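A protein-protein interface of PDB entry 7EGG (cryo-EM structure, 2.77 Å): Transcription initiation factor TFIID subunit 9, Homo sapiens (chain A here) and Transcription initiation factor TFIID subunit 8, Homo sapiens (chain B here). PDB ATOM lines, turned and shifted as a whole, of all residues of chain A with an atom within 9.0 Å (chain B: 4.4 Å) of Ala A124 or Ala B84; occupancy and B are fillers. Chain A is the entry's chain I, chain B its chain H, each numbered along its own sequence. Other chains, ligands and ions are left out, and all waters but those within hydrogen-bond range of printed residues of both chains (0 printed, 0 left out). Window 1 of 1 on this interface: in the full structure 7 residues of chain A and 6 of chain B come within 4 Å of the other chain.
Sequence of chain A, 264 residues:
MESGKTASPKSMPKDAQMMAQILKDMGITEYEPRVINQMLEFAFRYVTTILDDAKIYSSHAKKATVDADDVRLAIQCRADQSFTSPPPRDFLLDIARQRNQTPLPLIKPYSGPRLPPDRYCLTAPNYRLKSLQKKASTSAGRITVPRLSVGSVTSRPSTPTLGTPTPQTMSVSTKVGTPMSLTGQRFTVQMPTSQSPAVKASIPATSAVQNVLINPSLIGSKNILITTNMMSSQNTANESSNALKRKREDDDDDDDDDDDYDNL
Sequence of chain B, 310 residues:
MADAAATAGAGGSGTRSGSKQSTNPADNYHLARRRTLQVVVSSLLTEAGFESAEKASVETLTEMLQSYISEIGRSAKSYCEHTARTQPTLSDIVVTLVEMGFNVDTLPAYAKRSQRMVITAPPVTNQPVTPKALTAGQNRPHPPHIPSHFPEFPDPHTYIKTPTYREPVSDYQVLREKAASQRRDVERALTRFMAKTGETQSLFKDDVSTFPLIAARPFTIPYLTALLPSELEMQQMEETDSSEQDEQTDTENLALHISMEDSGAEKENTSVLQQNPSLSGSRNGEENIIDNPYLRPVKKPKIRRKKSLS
Among the printed residues, merely in contact across the chains: Asp A118 with Ala B84 (3.9 Å), Cys A121 with Ala B84 (3.3 Å), Leu A122 with Glu B81 (3.5 Å), Leu A122 with Ala B84 (3.1 Å) and Ala A124 with Arg B85 (3.7 Å).
Hydrophobic or aromatic side chains of chain B within 4 Å of the printed part of chain A: Ala B84.
Printed residues of chain A that touch a printed residue of chain B: Asp A118, Cys A121, Leu A122, Thr A123 and Ala A124.
Along chain A the printed residues that touch a printed residue of chain B span positions 118 to 124.
Among the printed residues, 7 pairs touch across the chains.
The backbone carbonyl oxygen (O) of Ala B84 sits at hydrogen-bond distance from the backbone NH (N) of Thr A123, at 3.3 Å.
N of Ala A124 lies close to O of Ala B84 (3.4 Å).
The backbone NH of Arg B85 sits at hydrogen-bond distance from the backbone carbonyl oxygen of Cys B80, 3.0 Å away.
The guanidinium group (NH2) of Arg B85 is in hydrogen-bond range of the side-chain hydroxyl (OG1) of Thr B83 (2.8 Å).
The backbone carbonyl oxygen of Pro A117 lies within hydrogen-bond range of the side-chain sulfur of Cys A121 (3.5 Å).
Ala A124 touches two residues of chain B.
Ala B84 touches just these residues of chain A: Asp A118 (3.9 Å), Cys A121 (3.3 Å), Leu A122 (3.1 Å), Thr A123 (3.3 Å) and Ala A124 (3.2 Å).
No residue of chain A comes within 4 Å of Thr B83.
Of the printed residues of chain B, Cys A121 touches Ala B84.
Of the printed residues of chain B, Thr A123 touches Ala B84 (3.3 Å).
Of the printed residues of chain A, Glu B81 touches Leu A122 (3.5 Å).
Cys B80 touches none of the printed residues of chain A.
Pro A117 touches none of the printed residues of chain B.
The nearest printed residue of chain B that does not touch Ala A124 is Thr B83 (4.5 Å).
The nearest residue of chain A that does not touch Ala B84 is Arg A119 (5.0 Å).
The nearest printed residue of chain A that does not touch Arg B85 is Asn A126 (4.01 Å).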
ATOM      1  N   PRO A 117     -23.862 -32.688  22.057  1.00  0.00           N
ATOM      2  CA  PRO A 117     -23.159 -31.663  21.275  1.00  0.00           C
ATOM      3  C   PRO A 117     -22.373 -30.702  22.157  1.00  0.00           C
ATOM      4  O   PRO A 117     -22.722 -30.458  23.314  1.00  0.00           O
ATOM      5  CB  PRO A 117     -24.294 -30.945  20.544  1.00  0.00           C
ATOM      6  CG  PRO A 117     -25.294 -32.004  20.329  1.00  0.00           C
ATOM      7  CD  PRO A 117     -25.215 -32.928  21.516  1.00  0.00           C
ATOM      8  N   ASP A 118     -21.294 -30.159  21.584  1.00  0.00           N
ATOM      9  CA  ASP A 118     -20.260 -29.485  22.363  1.00  0.00           C
ATOM     10  C   ASP A 118     -20.726 -28.175  22.984  1.00  0.00           C
ATOM     11  O   ASP A 118     -20.062 -27.672  23.896  1.00  0.00           O
ATOM     12  CB  ASP A 118     -19.033 -29.233  21.489  1.00  0.00           C
ATOM     13  CG  ASP A 118     -18.470 -30.507  20.895  1.00  0.00           C
ATOM     14  OD1 ASP A 118     -19.014 -31.592  21.188  1.00  0.00           O
ATOM     15  OD2 ASP A 118     -17.483 -30.424  20.137  1.00  0.00           O
ATOM     16  N   ARG A 119     -21.838 -27.612  22.521  1.00  0.00           N
ATOM     17  CA  ARG A 119     -22.429 -26.457  23.181  1.00  0.00           C
ATOM     18  C   ARG A 119     -23.304 -26.840  24.366  1.00  0.00           C
ATOM     19  O   ARG A 119     -23.833 -25.950  25.037  1.00  0.00           O
ATOM     20  CB  ARG A 119     -23.238 -25.637  22.180  1.00  0.00           C
ATOM     21  CG  ARG A 119     -24.294 -26.425  21.441  1.00  0.00           C
ATOM     22  CD  ARG A 119     -24.919 -25.585  20.347  1.00  0.00           C
ATOM     23  NE  ARG A 119     -26.327 -25.906  20.145  1.00  0.00           N
ATOM     24  CZ  ARG A 119     -27.322 -25.350  20.826  1.00  0.00           C
ATOM     25  NH1 ARG A 119     -28.576 -25.700  20.577  1.00  0.00           N
ATOM     26  NH2 ARG A 119     -27.063 -24.445  21.760  1.00  0.00           N
ATOM     27  N   TYR A 120     -23.470 -28.132  24.637  1.00  0.00           N
ATOM     28  CA  TYR A 120     -24.195 -28.607  25.805  1.00  0.00           C
ATOM     29  C   TYR A 120     -23.286 -29.274  26.824  1.00  0.00           C
ATOM     30  O   TYR A 120     -23.752 -29.633  27.910  1.00  0.00           O
ATOM     31  CB  TYR A 120     -25.298 -29.582  25.382  1.00  0.00           C
ATOM     32  CG  TYR A 120     -26.403 -28.932  24.585  1.00  0.00           C
ATOM     33  CD1 TYR A 120     -27.398 -28.200  25.216  1.00  0.00           C
ATOM     34  CD2 TYR A 120     -26.449 -29.047  23.203  1.00  0.00           C
ATOM     35  CE1 TYR A 120     -28.409 -27.605  24.495  1.00  0.00           C
ATOM     36  CE2 TYR A 120     -27.455 -28.453  22.472  1.00  0.00           C
ATOM     37  CZ  TYR A 120     -28.431 -27.732  23.125  1.00  0.00           C
ATOM     38  OH  TYR A 120     -29.440 -27.138  22.406  1.00  0.00           O
ATOM     39  N   CYS A 121     -22.008 -29.447  26.504  1.00  0.00           N
ATOM     40  CA  CYS A 121     -21.034 -30.029  27.408  1.00  0.00           C
ATOM     41  C   CYS A 121     -20.207 -28.928  28.062  1.00  0.00           C
ATOM     42  O   CYS A 121     -20.376 -27.740  27.786  1.00  0.00           O
ATOM     43  CB  CYS A 121     -20.138 -31.017  26.663  1.00  0.00           C
ATOM     44  SG  CYS A 121     -21.023 -32.296  25.768  1.00  0.00           S
ATOM     45  N   LEU A 122     -19.300 -29.332  28.944  1.00  0.00           N
ATOM     46  CA  LEU A 122     -18.390 -28.428  29.633  1.00  0.00           C
ATOM     47  C   LEU A 122     -16.947 -28.684  29.213  1.00  0.00           C
ATOM     48  O   LEU A 122     -16.037 -28.711  30.040  1.00  0.00           O
ATOM     49  CB  LEU A 122     -18.532 -28.558  31.145  1.00  0.00           C
ATOM     50  CG  LEU A 122     -19.936 -28.412  31.718  1.00  0.00           C
ATOM     51  CD1 LEU A 122     -19.917 -28.661  33.206  1.00  0.00           C
ATOM     52  CD2 LEU A 122     -20.491 -27.042  31.414  1.00  0.00           C
ATOM     53  N   THR A 123     -16.728 -28.893  27.920  1.00  0.00           N
ATOM     54  CA  THR A 123     -15.414 -29.228  27.377  1.00  0.00           C
ATOM     55  C   THR A 123     -15.018 -28.160  26.362  1.00  0.00           C
ATOM     56  O   THR A 123     -15.297 -28.294  25.171  1.00  0.00           O
ATOM     57  CB  THR A 123     -15.433 -30.609  26.749  1.00  0.00           C
ATOM     58  OG1 THR A 123     -16.516 -30.693  25.816  1.00  0.00           O
ATOM     59  CG2 THR A 123     -15.614 -31.669  27.810  1.00  0.00           C
ATOM     60  N   ALA A 124     -14.365 -27.111  26.836  1.00  0.00           N
ATOM     61  CA  ALA A 124     -13.879 -25.998  26.038  1.00  0.00           C
ATOM     62  C   ALA A 124     -12.406 -25.800  26.366  1.00  0.00           C
ATOM     63  O   ALA A 124     -11.919 -26.349  27.360  1.00  0.00           O
ATOM     64  CB  ALA A 124     -14.691 -24.729  26.337  1.00  0.00           C
ATOM     65  N   PRO A 125     -11.652 -25.062  25.531  1.00  0.00           N
ATOM     66  CA  PRO A 125     -10.213 -24.874  25.811  1.00  0.00           C
ATOM     67  C   PRO A 125      -9.867 -24.184  27.127  1.00  0.00           C
ATOM     68  O   PRO A 125      -8.719 -24.317  27.566  1.00  0.00           O
ATOM     69  CB  PRO A 125      -9.745 -24.041  24.616  1.00  0.00           C
ATOM     70  CG  PRO A 125     -10.571 -24.527  23.517  1.00  0.00           C
ATOM     71  CD  PRO A 125     -11.930 -24.789  24.104  1.00  0.00           C
ATOM     72  N   ASN A 126     -10.805 -23.461  27.752  1.00  0.00           N
ATOM     73  CA  ASN A 126     -10.788 -23.109  29.179  1.00  0.00           C
ATOM     74  C   ASN A 126      -9.561 -22.268  29.560  1.00  0.00           C
ATOM     75  O   ASN A 126      -8.675 -22.702  30.292  1.00  0.00           O
ATOM     76  CB  ASN A 126     -10.871 -24.377  30.035  1.00  0.00           C
ATOM     77  CG  ASN A 126     -11.350 -24.099  31.427  1.00  0.00           C
ATOM     78  OD1 ASN A 126     -11.684 -22.967  31.757  1.00  0.00           O
ATOM     79  ND2 ASN A 126     -11.392 -25.130  32.258  1.00  0.00           N
ATOM     80  N   TYR A 127      -9.538 -21.048  29.035  1.00  0.00           N
ATOM     81  CA  TYR A 127      -8.365 -20.184  29.056  1.00  0.00           C
ATOM     82  C   TYR A 127      -8.124 -19.575  30.443  1.00  0.00           C
ATOM     83  O   TYR A 127      -8.922 -19.725  31.369  1.00  0.00           O
ATOM     84  CB  TYR A 127      -8.518 -19.081  28.012  1.00  0.00           C
ATOM     85  CG  TYR A 127      -8.591 -19.590  26.591  1.00  0.00           C
ATOM     86  CD1 TYR A 127      -9.800 -19.992  26.030  1.00  0.00           C
ATOM     87  CD2 TYR A 127      -7.449 -19.667  25.808  1.00  0.00           C
ATOM     88  CE1 TYR A 127      -9.869 -20.450  24.738  1.00  0.00           C
ATOM     89  CE2 TYR A 127      -7.509 -20.129  24.510  1.00  0.00           C
ATOM     90  CZ  TYR A 127      -8.721 -20.519  23.982  1.00  0.00           C
ATOM     91  OH  TYR A 127      -8.787 -20.981  22.689  1.00  0.00           O
ATOM     92  N   CYS B  80     -19.681 -19.152  33.386  1.00  0.00           N
ATOM     93  CA  CYS B  80     -18.648 -19.838  32.620  1.00  0.00           C
ATOM     94  C   CYS B  80     -19.158 -21.159  32.062  1.00  0.00           C
ATOM     95  O   CYS B  80     -18.862 -21.501  30.913  1.00  0.00           O
ATOM     96  CB  CYS B  80     -17.401 -20.059  33.476  1.00  0.00           C
ATOM     97  SG  CYS B  80     -17.525 -21.355  34.716  1.00  0.00           S
ATOM     98  N   GLU B  81     -19.932 -21.908  32.855  1.00  0.00           N
ATOM     99  CA  GLU B  81     -20.489 -23.174  32.393  1.00  0.00           C
ATOM    100  C   GLU B  81     -21.573 -22.988  31.345  1.00  0.00           C
ATOM    101  O   GLU B  81     -21.860 -23.928  30.597  1.00  0.00           O
ATOM    102  CB  GLU B  81     -21.046 -23.967  33.568  1.00  0.00           C
ATOM    103  CG  GLU B  81     -19.980 -24.602  34.422  1.00  0.00           C
ATOM    104  CD  GLU B  81     -20.559 -25.435  35.533  1.00  0.00           C
ATOM    105  OE1 GLU B  81     -21.788 -25.368  35.740  1.00  0.00           O
ATOM    106  OE2 GLU B  81     -19.790 -26.156  36.200  1.00  0.00           O
ATOM    107  N   HIS B  82     -22.190 -21.808  31.282  1.00  0.00           N
ATOM    108  CA  HIS B  82     -23.059 -21.490  30.159  1.00  0.00           C
ATOM    109  C   HIS B  82     -22.263 -21.367  28.869  1.00  0.00           C
ATOM    110  O   HIS B  82     -22.777 -21.676  27.789  1.00  0.00           O
ATOM    111  CB  HIS B  82     -23.824 -20.200  30.441  1.00  0.00           C
ATOM    112  CG  HIS B  82     -24.812 -19.841  29.381  1.00  0.00           C
ATOM    113  ND1 HIS B  82     -25.951 -20.580  29.147  1.00  0.00           N
ATOM    114  CD2 HIS B  82     -24.834 -18.824  28.488  1.00  0.00           C
ATOM    115  CE1 HIS B  82     -26.632 -20.034  28.158  1.00  0.00           C
ATOM    116  NE2 HIS B  82     -25.976 -18.965  27.742  1.00  0.00           N
ATOM    117  N   THR B  83     -21.010 -20.926  28.963  1.00  0.00           N
ATOM    118  CA  THR B  83     -20.100 -20.846  27.829  1.00  0.00           C
ATOM    119  C   THR B  83     -19.219 -22.081  27.704  1.00  0.00           C
ATOM    120  O   THR B  83     -18.090 -21.979  27.204  1.00  0.00           O
ATOM    121  CB  THR B  83     -19.242 -19.589  27.939  1.00  0.00           C
ATOM    122  OG1 THR B  83     -18.410 -19.687  29.099  1.00  0.00           O
ATOM    123  CG2 THR B  83     -20.122 -18.362  28.070  1.00  0.00           C
ATOM    124  N   ALA B  84     -19.700 -23.226  28.200  1.00  0.00           N
ATOM    125  CA  ALA B  84     -19.116 -24.562  28.047  1.00  0.00           C
ATOM    126  C   ALA B  84     -17.753 -24.713  28.714  1.00  0.00           C
ATOM    127  O   ALA B  84     -17.018 -25.645  28.397  1.00  0.00           O
ATOM    128  CB  ALA B  84     -19.027 -24.975  26.572  1.00  0.00           C
ATOM    129  N   ARG B  85     -17.399 -23.845  29.655  1.00  0.00           N
ATOM    130  CA  ARG B  85     -16.122 -23.932  30.352  1.00  0.00           C
ATOM    131  C   ARG B  85     -16.334 -24.435  31.775  1.00  0.00           C
ATOM    132  O   ARG B  85     -17.460 -24.558  32.254  1.00  0.00           O
ATOM    133  CB  ARG B  85     -15.415 -22.574  30.355  1.00  0.00           C
ATOM    134  CG  ARG B  85     -14.842 -22.189  29.009  1.00  0.00           C
ATOM    135  CD  ARG B  85     -14.136 -20.853  29.048  1.00  0.00           C
ATOM    136  NE  ARG B  85     -15.064 -19.739  28.915  1.00  0.00           N
ATOM    137  CZ  ARG B  85     -15.448 -18.968  29.924  1.00  0.00           C
ATOM    138  NH1 ARG B  85     -14.989 -19.193  31.145  1.00  0.00           N
ATOM    139  NH2 ARG B  85     -16.296 -17.973  29.713  1.00  0.00           N
